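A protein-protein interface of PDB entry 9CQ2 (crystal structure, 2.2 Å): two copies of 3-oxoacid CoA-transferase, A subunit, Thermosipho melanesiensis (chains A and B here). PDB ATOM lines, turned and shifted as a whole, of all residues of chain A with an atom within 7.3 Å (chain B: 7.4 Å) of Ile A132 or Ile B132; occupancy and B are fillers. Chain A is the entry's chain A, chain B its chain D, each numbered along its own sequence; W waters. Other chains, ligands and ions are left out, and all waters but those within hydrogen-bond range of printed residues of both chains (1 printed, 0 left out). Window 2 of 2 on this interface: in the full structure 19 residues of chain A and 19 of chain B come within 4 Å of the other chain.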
ATOM      1  N   GLY A 113     -19.990  -3.845  13.242  1.00  0.00           N
ATOM      2  CA  GLY A 113     -19.482  -5.041  12.585  1.00  0.00           C
ATOM      3  C   GLY A 113     -18.441  -4.792  11.516  1.00  0.00           C
ATOM      4  O   GLY A 113     -17.882  -5.743  10.954  1.00  0.00           O
ATOM      5  N   ILE A 115     -16.689  -1.200   8.876  1.00  0.00           N
ATOM      6  CA  ILE A 115     -16.831   0.133   8.306  1.00  0.00           C
ATOM      7  C   ILE A 115     -16.360   0.084   6.864  1.00  0.00           C
ATOM      8  O   ILE A 115     -15.450  -0.685   6.523  1.00  0.00           O
ATOM      9  CB  ILE A 115     -16.046   1.208   9.087  1.00  0.00           C
ATOM     10  CG1 ILE A 115     -14.600   0.786   9.392  1.00  0.00           C
ATOM     11  CG2 ILE A 115     -16.658   1.439  10.451  1.00  0.00           C
ATOM     12  CD1 ILE A 115     -13.623   1.340   8.459  1.00  0.00           C
ATOM     13  N   LEU A 116     -16.997   0.920   6.019  1.00  0.00           N
ATOM     14  CA  LEU A 116     -16.660   1.047   4.601  1.00  0.00           C
ATOM     15  C   LEU A 116     -15.776   2.266   4.397  1.00  0.00           C
ATOM     16  O   LEU A 116     -16.177   3.378   4.726  1.00  0.00           O
ATOM     17  CB  LEU A 116     -17.919   1.188   3.741  1.00  0.00           C
ATOM     18  CG  LEU A 116     -18.718  -0.052   3.331  1.00  0.00           C
ATOM     19  CD1 LEU A 116     -19.155  -0.830   4.548  1.00  0.00           C
ATOM     20  CD2 LEU A 116     -19.935   0.329   2.464  1.00  0.00           C
ATOM     21  N   THR A 117     -14.605   2.064   3.818  1.00  0.00           N
ATOM     22  CA  THR A 117     -13.713   3.171   3.598  1.00  0.00           C
ATOM     23  C   THR A 117     -13.161   3.188   2.179  1.00  0.00           C
ATOM     24  O   THR A 117     -12.730   2.154   1.658  1.00  0.00           O
ATOM     25  CB  THR A 117     -12.522   3.145   4.541  1.00  0.00           C
ATOM     26  OG1 THR A 117     -11.721   4.329   4.338  1.00  0.00           O
ATOM     27  CG2 THR A 117     -11.641   1.956   4.276  1.00  0.00           C
ATOM     28  N   VAL A 121      -8.653   1.577  -1.670  1.00  0.00           N
ATOM     29  CA  VAL A 121      -9.265   1.035  -2.878  1.00  0.00           C
ATOM     30  C   VAL A 121      -8.264   1.076  -4.044  1.00  0.00           C
ATOM     31  O   VAL A 121      -7.539   2.060  -4.248  1.00  0.00           O
ATOM     32  CB  VAL A 121     -10.539   1.824  -3.217  1.00  0.00           C
ATOM     33  CG1 VAL A 121     -10.962   1.551  -4.643  1.00  0.00           C
ATOM     34  CG2 VAL A 121     -11.681   1.489  -2.291  1.00  0.00           C
ATOM     35  N   LYS A 129     -10.247  -8.119   0.588  1.00  0.00           N
ATOM     36  CA  LYS A 129     -11.311  -7.321   1.174  1.00  0.00           C
ATOM     37  C   LYS A 129     -12.567  -7.449   0.328  1.00  0.00           C
ATOM     38  O   LYS A 129     -12.497  -7.466  -0.902  1.00  0.00           O
ATOM     39  CB  LYS A 129     -10.923  -5.844   1.275  1.00  0.00           C
ATOM     40  CG  LYS A 129      -9.596  -5.579   1.989  1.00  0.00           C
ATOM     41  CD  LYS A 129      -9.773  -5.582   3.500  1.00  0.00           C
ATOM     42  CE  LYS A 129      -8.436  -5.577   4.183  1.00  0.00           C
ATOM     43  NZ  LYS A 129      -7.707  -4.330   3.783  1.00  0.00           N
ATOM     44  N   LYS A 130     -13.717  -7.570   0.986  1.00  0.00           N
ATOM     45  CA  LYS A 130     -14.962  -7.367   0.268  1.00  0.00           C
ATOM     46  C   LYS A 130     -15.001  -5.924  -0.193  1.00  0.00           C
ATOM     47  O   LYS A 130     -14.606  -5.012   0.544  1.00  0.00           O
ATOM     48  CB  LYS A 130     -16.180  -7.699   1.134  1.00  0.00           C
ATOM     49  CG  LYS A 130     -17.429  -8.052   0.332  1.00  0.00           C
ATOM     50  CD  LYS A 130     -18.687  -8.163   1.190  1.00  0.00           C
ATOM     51  CE  LYS A 130     -18.758  -9.520   1.888  1.00  0.00           C
ATOM     52  NZ  LYS A 130     -20.154 -10.026   2.055  1.00  0.00           N
ATOM     53  N   VAL A 131     -15.415  -5.730  -1.434  1.00  0.00           N
ATOM     54  CA  VAL A 131     -15.646  -4.409  -1.991  1.00  0.00           C
ATOM     55  C   VAL A 131     -17.139  -4.166  -2.062  1.00  0.00           C
ATOM     56  O   VAL A 131     -17.911  -5.041  -2.478  1.00  0.00           O
ATOM     57  CB  VAL A 131     -15.005  -4.282  -3.378  1.00  0.00           C
ATOM     58  CG1 VAL A 131     -15.483  -3.010  -4.013  1.00  0.00           C
ATOM     59  CG2 VAL A 131     -13.493  -4.306  -3.283  1.00  0.00           C
ATOM     60  N   ILE A 132     -17.556  -2.974  -1.660  1.00  0.00           N
ATOM     61  CA  ILE A 132     -18.964  -2.617  -1.660  1.00  0.00           C
ATOM     62  C   ILE A 132     -19.112  -1.276  -2.369  1.00  0.00           C
ATOM     63  O   ILE A 132     -18.355  -0.330  -2.101  1.00  0.00           O
ATOM     64  CB  ILE A 132     -19.536  -2.550  -0.235  1.00  0.00           C
ATOM     65  CG1 ILE A 132     -19.497  -3.941   0.402  1.00  0.00           C
ATOM     66  CG2 ILE A 132     -20.970  -2.037  -0.249  1.00  0.00           C
ATOM     67  CD1 ILE A 132     -19.808  -3.921   1.897  1.00  0.00           C
ATOM     68  N   GLU A 133     -20.074  -1.200  -3.280  1.00  0.00           N
ATOM     69  CA  GLU A 133     -20.356   0.030  -3.993  1.00  0.00           C
ATOM     70  C   GLU A 133     -21.575   0.655  -3.364  1.00  0.00           C
ATOM     71  O   GLU A 133     -22.544  -0.043  -3.060  1.00  0.00           O
ATOM     72  CB  GLU A 133     -20.592  -0.205  -5.480  1.00  0.00           C
ATOM     73  CG  GLU A 133     -19.450   0.355  -6.293  1.00  0.00           C
ATOM     74  CD  GLU A 133     -19.459  -0.098  -7.741  1.00  0.00           C
ATOM     75  OE1 GLU A 133     -20.504   0.068  -8.406  1.00  0.00           O
ATOM     76  OE2 GLU A 133     -18.439  -0.639  -8.211  1.00  0.00           O
ATOM     77  N   VAL A 134     -21.501   1.960  -3.140  1.00  0.00           N
ATOM     78  CA  VAL A 134     -22.579   2.734  -2.538  1.00  0.00           C
ATOM     79  C   VAL A 134     -22.703   3.971  -3.402  1.00  0.00           C
ATOM     80  O   VAL A 134     -21.750   4.754  -3.497  1.00  0.00           O
ATOM     81  CB  VAL A 134     -22.302   3.111  -1.065  1.00  0.00           C
ATOM     82  CG1 VAL A 134     -23.378   4.047  -0.503  1.00  0.00           C
ATOM     83  CG2 VAL A 134     -22.201   1.859  -0.179  1.00  0.00           C
ATOM     84  N   GLY A 136     -22.640   4.271  -6.636  1.00  0.00           N
ATOM     85  CA  GLY A 136     -21.625   4.231  -7.654  1.00  0.00           C
ATOM     86  C   GLY A 136     -20.196   4.140  -7.167  1.00  0.00           C
ATOM     87  O   GLY A 136     -19.341   3.661  -7.924  1.00  0.00           O
ATOM     88  N   LYS A 137     -19.897   4.583  -5.936  1.00  0.00           N
ATOM     89  CA  LYS A 137     -18.524   4.612  -5.433  1.00  0.00           C
ATOM     90  C   LYS A 137     -18.155   3.317  -4.710  1.00  0.00           C
ATOM     91  O   LYS A 137     -18.994   2.685  -4.050  1.00  0.00           O
ATOM     92  CB  LYS A 137     -18.304   5.806  -4.494  1.00  0.00           C
ATOM     93  CG  LYS A 137     -16.823   6.008  -4.153  1.00  0.00           C
ATOM     94  CD  LYS A 137     -16.458   7.401  -3.582  1.00  0.00           C
ATOM     95  CE  LYS A 137     -14.896   7.520  -3.466  1.00  0.00           C
ATOM     96  NZ  LYS A 137     -14.315   8.574  -2.541  1.00  0.00           N
ATOM     97  N   LYS A 138     -16.886   2.930  -4.862  1.00  0.00           N
ATOM     98  CA  LYS A 138     -16.341   1.701  -4.304  1.00  0.00           C
ATOM     99  C   LYS A 138     -15.758   1.991  -2.928  1.00  0.00           C
ATOM    100  O   LYS A 138     -15.136   3.036  -2.716  1.00  0.00           O
ATOM    101  CB  LYS A 138     -15.243   1.116  -5.208  1.00  0.00           C
ATOM    102  CG  LYS A 138     -15.711   0.182  -6.348  1.00  0.00           C
ATOM    103  CD  LYS A 138     -14.543  -0.400  -7.181  1.00  0.00           C
ATOM    104  CE  LYS A 138     -13.517  -1.125  -6.319  1.00  0.00           C
ATOM    105  NZ  LYS A 138     -12.604  -2.026  -7.083  1.00  0.00           N
ATOM    106  N   TYR A 139     -15.966   1.060  -2.001  1.00  0.00           N
ATOM    107  CA  TYR A 139     -15.362   1.130  -0.683  1.00  0.00           C
ATOM    108  C   TYR A 139     -14.890  -0.259  -0.302  1.00  0.00           C
ATOM    109  O   TYR A 139     -15.473  -1.258  -0.719  1.00  0.00           O
ATOM    110  CB  TYR A 139     -16.352   1.614   0.378  1.00  0.00           C
ATOM    111  CG  TYR A 139     -16.957   2.961   0.102  1.00  0.00           C
ATOM    112  CD1 TYR A 139     -16.329   4.122   0.526  1.00  0.00           C
ATOM    113  CD2 TYR A 139     -18.164   3.070  -0.582  1.00  0.00           C
ATOM    114  CE1 TYR A 139     -16.895   5.365   0.287  1.00  0.00           C
ATOM    115  CE2 TYR A 139     -18.739   4.307  -0.834  1.00  0.00           C
ATOM    116  CZ  TYR A 139     -18.090   5.452  -0.401  1.00  0.00           C
ATOM    117  OH  TYR A 139     -18.633   6.682  -0.656  1.00  0.00           O
ATOM    118  N   LEU A 140     -13.842  -0.307   0.508  1.00  0.00           N
ATOM    119  CA  LEU A 140     -13.395  -1.541   1.131  1.00  0.00           C
ATOM    120  C   LEU A 140     -14.123  -1.729   2.460  1.00  0.00           C
ATOM    121  O   LEU A 140     -14.178  -0.808   3.291  1.00  0.00           O
ATOM    122  CB  LEU A 140     -11.888  -1.511   1.375  1.00  0.00           C
ATOM    123  CG  LEU A 140     -10.969  -1.219   0.188  1.00  0.00           C
ATOM    124  CD1 LEU A 140      -9.500  -1.314   0.643  1.00  0.00           C
ATOM    125  CD2 LEU A 140     -11.281  -2.176  -0.991  1.00  0.00           C
ATOM    126  N   LEU A 141     -14.693  -2.915   2.649  1.00  0.00           N
ATOM    127  CA  LEU A 141     -15.196  -3.315   3.952  1.00  0.00           C
ATOM    128  C   LEU A 141     -14.010  -3.692   4.822  1.00  0.00           C
ATOM    129  O   LEU A 141     -13.237  -4.598   4.485  1.00  0.00           O
ATOM    130  CB  LEU A 141     -16.157  -4.479   3.843  1.00  0.00           C
ATOM    131  CG  LEU A 141     -16.626  -5.071   5.174  1.00  0.00           C
ATOM    132  CD1 LEU A 141     -17.461  -4.069   5.913  1.00  0.00           C
ATOM    133  CD2 LEU A 141     -17.463  -6.304   4.988  1.00  0.00           C
ATOM    134  N   GLU A 142     -13.855  -2.969   5.916  1.00  0.00           N
ATOM    135  CA  GLU A 142     -12.762  -3.165   6.856  1.00  0.00           C
ATOM    136  C   GLU A 142     -13.370  -3.592   8.179  1.00  0.00           C
ATOM    137  O   GLU A 142     -14.438  -3.121   8.575  1.00  0.00           O
ATOM    138  CB  GLU A 142     -11.935  -1.907   6.957  1.00  0.00           C
ATOM    139  CG  GLU A 142     -11.200  -1.613   5.659  1.00  0.00           C
ATOM    140  CD  GLU A 142      -9.907  -2.417   5.512  1.00  0.00           C
ATOM    141  OE1 GLU A 142      -9.655  -3.330   6.336  1.00  0.00           O
ATOM    142  OE2 GLU A 142      -9.118  -2.124   4.583  1.00  0.00           O
ATOM    143  N   LEU A 143     -12.717  -4.513   8.839  1.00  0.00           N
ATOM    144  CA  LEU A 143     -13.405  -5.254   9.883  1.00  0.00           C
ATOM    145  C   LEU A 143     -12.885  -4.926  11.279  1.00  0.00           C
ATOM    146  O   LEU A 143     -11.712  -4.577  11.458  1.00  0.00           O
ATOM    147  CB  LEU A 143     -13.280  -6.765   9.634  1.00  0.00           C
ATOM    148  CG  LEU A 143     -13.877  -7.298   8.337  1.00  0.00           C
ATOM    149  CD1 LEU A 143     -13.433  -8.732   8.215  1.00  0.00           C
ATOM    150  CD2 LEU A 143     -15.376  -7.149   8.358  1.00  0.00           C
ATOM    151  N   GLY B 113     -18.056   5.211   3.773  1.00  0.00           N
ATOM    152  CA  GLY B 113     -19.159   4.848   2.901  1.00  0.00           C
ATOM    153  C   GLY B 113     -20.338   4.241   3.608  1.00  0.00           C
ATOM    154  O   GLY B 113     -21.387   4.038   2.992  1.00  0.00           O
ATOM    155  N   ILE B 115     -21.481   2.023   7.655  1.00  0.00           N
ATOM    156  CA  ILE B 115     -21.094   1.233   8.816  1.00  0.00           C
ATOM    157  C   ILE B 115     -22.074   0.072   8.969  1.00  0.00           C
ATOM    158  O   ILE B 115     -23.237   0.177   8.574  1.00  0.00           O
ATOM    159  CB  ILE B 115     -21.076   2.110  10.083  1.00  0.00           C
ATOM    160  CG1 ILE B 115     -22.364   2.921  10.179  1.00  0.00           C
ATOM    161  CG2 ILE B 115     -19.909   3.133  10.041  1.00  0.00           C
ATOM    162  CD1 ILE B 115     -23.382   2.249  10.967  1.00  0.00           C
ATOM    163  N   LEU B 116     -21.603  -1.038   9.567  1.00  0.00           N
ATOM    164  CA  LEU B 116     -22.462  -2.177   9.886  1.00  0.00           C
ATOM    165  C   LEU B 116     -22.785  -2.197  11.374  1.00  0.00           C
ATOM    166  O   LEU B 116     -21.881  -2.150  12.215  1.00  0.00           O
ATOM    167  CB  LEU B 116     -21.810  -3.508   9.503  1.00  0.00           C
ATOM    168  CG  LEU B 116     -20.928  -3.641   8.251  1.00  0.00           C
ATOM    169  CD1 LEU B 116     -20.590  -5.114   7.974  1.00  0.00           C
ATOM    170  CD2 LEU B 116     -21.528  -3.000   7.040  1.00  0.00           C
ATOM    171  N   THR B 117     -24.071  -2.283  11.689  1.00  0.00           N
ATOM    172  CA  THR B 117     -24.477  -2.300  13.066  1.00  0.00           C
ATOM    173  C   THR B 117     -25.440  -3.448  13.347  1.00  0.00           C
ATOM    174  O   THR B 117     -26.336  -3.719  12.545  1.00  0.00           O
ATOM    175  CB  THR B 117     -25.152  -0.994  13.451  1.00  0.00           C
ATOM    176  OG1 THR B 117     -25.616  -1.078  14.800  1.00  0.00           O
ATOM    177  CG2 THR B 117     -26.338  -0.686  12.507  1.00  0.00           C
ATOM    178  N   VAL B 121     -31.364  -5.306  13.524  1.00  0.00           N
ATOM    179  CA  VAL B 121     -31.462  -6.584  12.821  1.00  0.00           C
ATOM    180  C   VAL B 121     -32.714  -7.321  13.300  1.00  0.00           C
ATOM    181  O   VAL B 121     -33.017  -7.360  14.500  1.00  0.00           O
ATOM    182  CB  VAL B 121     -30.203  -7.436  13.055  1.00  0.00           C
ATOM    183  CG1 VAL B 121     -30.481  -8.879  12.657  1.00  0.00           C
ATOM    184  CG2 VAL B 121     -28.976  -6.914  12.302  1.00  0.00           C
ATOM    185  N   LYS B 129     -32.719  -2.615   3.917  1.00  0.00           N
ATOM    186  CA  LYS B 129     -31.305  -2.539   4.245  1.00  0.00           C
ATOM    187  C   LYS B 129     -30.587  -3.757   3.681  1.00  0.00           C
ATOM    188  O   LYS B 129     -31.134  -4.867   3.679  1.00  0.00           O
ATOM    189  CB  LYS B 129     -31.065  -2.451   5.766  1.00  0.00           C
ATOM    190  CG  LYS B 129     -31.796  -1.321   6.466  1.00  0.00           C
ATOM    191  CD  LYS B 129     -31.117   0.070   6.285  1.00  0.00           C
ATOM    192  CE  LYS B 129     -32.068   1.185   6.736  1.00  0.00           C
ATOM    193  NZ  LYS B 129     -32.361   1.146   8.228  1.00  0.00           N
ATOM    194  N   LYS B 130     -29.371  -3.537   3.191  1.00  0.00           N
ATOM    195  CA  LYS B 130     -28.491  -4.649   2.888  1.00  0.00           C
ATOM    196  C   LYS B 130     -28.034  -5.288   4.190  1.00  0.00           C
ATOM    197  O   LYS B 130     -27.644  -4.588   5.129  1.00  0.00           O
ATOM    198  CB  LYS B 130     -27.294  -4.183   2.075  1.00  0.00           C
ATOM    199  CG  LYS B 130     -26.201  -5.233   2.007  1.00  0.00           C
ATOM    200  CD  LYS B 130     -25.048  -4.830   1.085  1.00  0.00           C
ATOM    201  CE  LYS B 130     -25.058  -5.598  -0.228  1.00  0.00           C
ATOM    202  NZ  LYS B 130     -24.348  -6.893  -0.132  1.00  0.00           N
ATOM    203  N   VAL B 131     -28.125  -6.613   4.269  1.00  0.00           N
ATOM    204  CA  VAL B 131     -27.644  -7.366   5.418  1.00  0.00           C
ATOM    205  C   VAL B 131     -26.292  -7.967   5.069  1.00  0.00           C
ATOM    206  O   VAL B 131     -26.121  -8.546   3.987  1.00  0.00           O
ATOM    207  CB  VAL B 131     -28.645  -8.458   5.825  1.00  0.00           C
ATOM    208  CG1 VAL B 131     -28.095  -9.253   7.016  1.00  0.00           C
ATOM    209  CG2 VAL B 131     -29.993  -7.835   6.133  1.00  0.00           C
ATOM    210  N   ILE B 132     -25.327  -7.835   5.982  1.00  0.00           N
ATOM    211  CA  ILE B 132     -23.988  -8.381   5.800  1.00  0.00           C
ATOM    212  C   ILE B 132     -23.634  -9.230   7.005  1.00  0.00           C
ATOM    213  O   ILE B 132     -23.859  -8.824   8.154  1.00  0.00           O
ATOM    214  CB  ILE B 132     -22.924  -7.292   5.591  1.00  0.00           C
ATOM    215  CG1 ILE B 132     -23.351  -6.396   4.428  1.00  0.00           C
ATOM    216  CG2 ILE B 132     -21.601  -7.933   5.295  1.00  0.00           C
ATOM    217  CD1 ILE B 132     -22.297  -5.403   3.994  1.00  0.00           C
ATOM    218  N   GLU B 133     -23.101 -10.413   6.732  1.00  0.00           N
ATOM    219  CA  GLU B 133     -22.725 -11.377   7.744  1.00  0.00           C
ATOM    220  C   GLU B 133     -21.221 -11.309   7.908  1.00  0.00           C
ATOM    221  O   GLU B 133     -20.476 -11.398   6.925  1.00  0.00           O
ATOM    222  CB  GLU B 133     -23.163 -12.792   7.358  1.00  0.00           C
ATOM    223  CG  GLU B 133     -23.371 -13.711   8.556  1.00  0.00           C
ATOM    224  CD  GLU B 133     -24.563 -14.640   8.397  1.00  0.00           C
ATOM    225  OE1 GLU B 133     -25.595 -14.222   7.829  1.00  0.00           O
ATOM    226  OE2 GLU B 133     -24.482 -15.791   8.863  1.00  0.00           O
ATOM    227  N   VAL B 134     -20.789 -11.101   9.140  1.00  0.00           N
ATOM    228  CA  VAL B 134     -19.379 -11.083   9.497  1.00  0.00           C
ATOM    229  C   VAL B 134     -19.255 -12.007  10.686  1.00  0.00           C
ATOM    230  O   VAL B 134     -19.919 -11.789  11.710  1.00  0.00           O
ATOM    231  CB  VAL B 134     -18.871  -9.673   9.853  1.00  0.00           C
ATOM    232  CG1 VAL B 134     -17.432  -9.716  10.409  1.00  0.00           C
ATOM    233  CG2 VAL B 134     -18.978  -8.748   8.651  1.00  0.00           C
ATOM    234  N   GLU B 135     -18.410 -13.027  10.564  1.00  0.00           N
ATOM    235  CA  GLU B 135     -18.200 -13.977  11.660  1.00  0.00           C
ATOM    236  C   GLU B 135     -19.538 -14.549  12.133  1.00  0.00           C
ATOM    237  O   GLU B 135     -19.806 -14.674  13.334  1.00  0.00           O
ATOM    238  CB  GLU B 135     -17.440 -13.327  12.820  1.00  0.00           C
ATOM    239  CG  GLU B 135     -15.983 -12.997  12.501  1.00  0.00           C
ATOM    240  CD  GLU B 135     -15.179 -14.141  11.822  1.00  0.00           C
ATOM    241  OE1 GLU B 135     -15.709 -15.148  11.282  1.00  0.00           O
ATOM    242  OE2 GLU B 135     -13.952 -14.014  11.802  1.00  0.00           O
ATOM    243  N   GLY B 136     -20.393 -14.910  11.172  1.00  0.00           N
ATOM    244  CA  GLY B 136     -21.682 -15.502  11.458  1.00  0.00           C
ATOM    245  C   GLY B 136     -22.689 -14.606  12.143  1.00  0.00           C
ATOM    246  O   GLY B 136     -23.832 -15.043  12.349  1.00  0.00           O
ATOM    247  N   LYS B 137     -22.319 -13.380  12.514  1.00  0.00           N
ATOM    248  CA  LYS B 137     -23.275 -12.412  13.044  1.00  0.00           C
ATOM    249  C   LYS B 137     -23.800 -11.514  11.915  1.00  0.00           C
ATOM    250  O   LYS B 137     -23.065 -11.158  10.983  1.00  0.00           O
ATOM    251  CB  LYS B 137     -22.644 -11.591  14.172  1.00  0.00           C
ATOM    252  CG  LYS B 137     -23.699 -10.814  14.949  1.00  0.00           C
ATOM    253  CD  LYS B 137     -23.198 -10.104  16.220  1.00  0.00           C
ATOM    254  CE  LYS B 137     -24.402  -9.480  16.958  1.00  0.00           C
ATOM    255  NZ  LYS B 137     -24.097  -8.710  18.202  1.00  0.00           N
ATOM    256  N   LYS B 138     -25.097 -11.207  11.966  1.00  0.00           N
ATOM    257  CA  LYS B 138     -25.731 -10.379  10.947  1.00  0.00           C
ATOM    258  C   LYS B 138     -25.658  -8.903  11.345  1.00  0.00           C
ATOM    259  O   LYS B 138     -25.864  -8.553  12.511  1.00  0.00           O
ATOM    260  CB  LYS B 138     -27.193 -10.789  10.737  1.00  0.00           C
ATOM    261  CG  LYS B 138     -27.387 -12.115  10.017  1.00  0.00           C
ATOM    262  CD  LYS B 138     -28.848 -12.535   9.932  1.00  0.00           C
ATOM    263  CE  LYS B 138     -29.006 -13.750   9.041  1.00  0.00           C
ATOM    264  NZ  LYS B 138     -28.742 -13.498   7.618  1.00  0.00           N
ATOM    265  N   TYR B 139     -25.363  -8.043  10.364  1.00  0.00           N
ATOM    266  CA  TYR B 139     -25.356  -6.602  10.555  1.00  0.00           C
ATOM    267  C   TYR B 139     -26.182  -5.956   9.456  1.00  0.00           C
ATOM    268  O   TYR B 139     -26.260  -6.473   8.342  1.00  0.00           O
ATOM    269  CB  TYR B 139     -23.928  -6.063  10.536  1.00  0.00           C
ATOM    270  CG  TYR B 139     -23.055  -6.653  11.630  1.00  0.00           C
ATOM    271  CD1 TYR B 139     -23.042  -6.097  12.905  1.00  0.00           C
ATOM    272  CD2 TYR B 139     -22.254  -7.761  11.390  1.00  0.00           C
ATOM    273  CE1 TYR B 139     -22.244  -6.638  13.920  1.00  0.00           C
ATOM    274  CE2 TYR B 139     -21.446  -8.309  12.393  1.00  0.00           C
ATOM    275  CZ  TYR B 139     -21.446  -7.744  13.658  1.00  0.00           C
ATOM    276  OH  TYR B 139     -20.652  -8.277  14.652  1.00  0.00           O
ATOM    277  N   LEU B 140     -26.844  -4.852   9.799  1.00  0.00           N
ATOM    278  CA  LEU B 140     -27.393  -3.942   8.807  1.00  0.00           C
ATOM    279  C   LEU B 140     -26.318  -2.983   8.292  1.00  0.00           C
ATOM    280  O   LEU B 140     -25.539  -2.424   9.072  1.00  0.00           O
ATOM    281  CB  LEU B 140     -28.541  -3.136   9.397  1.00  0.00           C
ATOM    282  CG  LEU B 140     -29.660  -3.943  10.022  1.00  0.00           C
ATOM    283  CD1 LEU B 140     -30.826  -3.014  10.430  1.00  0.00           C
ATOM    284  CD2 LEU B 140     -30.145  -5.075   9.089  1.00  0.00           C
ATOM    285  N   LEU B 141     -26.289  -2.791   6.977  1.00  0.00           N
ATOM    286  CA  LEU B 141     -25.446  -1.783   6.356  1.00  0.00           C
ATOM    287  C   LEU B 141     -26.233  -0.488   6.396  1.00  0.00           C
ATOM    288  O   LEU B 141     -27.353  -0.414   5.876  1.00  0.00           O
ATOM    289  CB  LEU B 141     -25.064  -2.151   4.925  1.00  0.00           C
ATOM    290  CG  LEU B 141     -24.310  -1.025   4.194  1.00  0.00           C
ATOM    291  CD1 LEU B 141     -23.029  -0.665   4.916  1.00  0.00           C
ATOM    292  CD2 LEU B 141     -23.952  -1.378   2.787  1.00  0.00           C
ATOM    293  N   LEU B 143     -26.152   3.745   5.962  1.00  0.00           N
ATOM    294  CA  LEU B 143     -25.439   4.572   5.007  1.00  0.00           C
ATOM    295  C   LEU B 143     -25.249   6.006   5.506  1.00  0.00           C
ATOM    296  O   LEU B 143     -26.039   6.505   6.320  1.00  0.00           O
ATOM    297  CB  LEU B 143     -26.205   4.569   3.684  1.00  0.00           C
ATOM    298  CG  LEU B 143     -26.260   3.197   3.005  1.00  0.00           C
ATOM    299  CD1 LEU B 143     -27.029   3.393   1.731  1.00  0.00           C
ATOM    300  CD2 LEU B 143     -24.918   2.649   2.719  1.00  0.00           C
HETATM  301  O   HOH W   1     -22.594 -11.434   3.874  1.00  0.00           O
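N of Gly B113 is in hydrogen-bond range of O of Leu A116 (2.8 Å).
The backbone NH of Gly A113 is in hydrogen-bond range of the backbone carbonyl oxygen of Leu B116 (2.7 Å).
Water W1 bridges the backbone NH of Glu B133 (3.1 Å) and the side-chain amino group of Lys A130 (3.4 Å).
The backbone carbonyl oxygen of Lys A130 lies within hydrogen-bond range of the backbone NH of Leu A141.
The backbone NH (N) of Tyr B139 sits at hydrogen-bond distance from the backbone carbonyl oxygen (O) of Ile B132, at 2.8 Å.
The backbone NH (N) of Glu A142 is in hydrogen-bond range of the backbone carbonyl oxygen (O) of Ile A115.
The backbone NH (N) of Tyr A139 is in hydrogen-bond range of the backbone carbonyl oxygen (O) of Ile A132 (2.8 Å).
O of Lys B130 is in hydrogen-bond range of N of Leu B141 (2.9 Å).
Among the printed residues, merely in contact across the chains: Gly A113 with Val B134, Gly A113 with Tyr B139, Ile A115 with Ile B115, Leu A116 with Leu B141, Ile A132 with Ile B132, Val A134 with Gly B113, Val A134 with Leu B143, Tyr A139 with Gly B113, Leu A141 with Leu B116 and Leu A143 with Val B134.
Hydrophobic or aromatic side chains of chain A within 4 Å of the printed part of chain B: Ile A115, Leu A116, Ile A132, Val A134, Tyr A139, Leu A141 and Leu A143.
Of the 19 printed residues of chain B, 8 touch a printed residue of chain A.
Printed residues of chain B that touch a printed residue of chain A: Gly B113, Ile B115, Leu B116, Ile B132, Val B134, Tyr B139, Leu B141 and Leu B143.
Of chain B, only Ile B132 (3.6 Å) comes within 4 Å of Ile A132.
Printed residues of chain B within 4 Å of Val A134: Gly B113 and Leu B143.
Of the printed residues of chain B, Tyr A139 touches Gly B113 (3.5 Å).
Of the printed residues of chain B, Leu A141 touches Leu B116.
Of the printed residues of chain A, Gly B113 touches Leu A116, Val A134 and Tyr A139.
Of chain A, only Ile A132 (3.6 Å) comes within 4 Å of Ile B132.
Printed residues of chain A within 4 Å of Leu B143: Val A134 (3.8 Å).
The nearest printed residue of chain A that does not touch Tyr B139 is Leu A143 (7.4 Å).
Gly A113 touches Leu B116, and with the chains exchanged Leu A116 touches Gly B113.
Ile B115 touches its own counterpart, Ile A115.
Leu A116 touches Leu B141, and with the chains exchanged Leu A141 touches Leu B116.
Ile A132 touches its own counterpart, Ile B132.
Positions printed for both chains: 113, 115, 116, 117, 121, 129, 130, 131, 132, 133, 134, 136, 137, 138, 139, 140, 141 and 143.
Of the 12 pairs that touch across the chains among the printed residues, 12 have their exchanged pair printed and touching as well.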
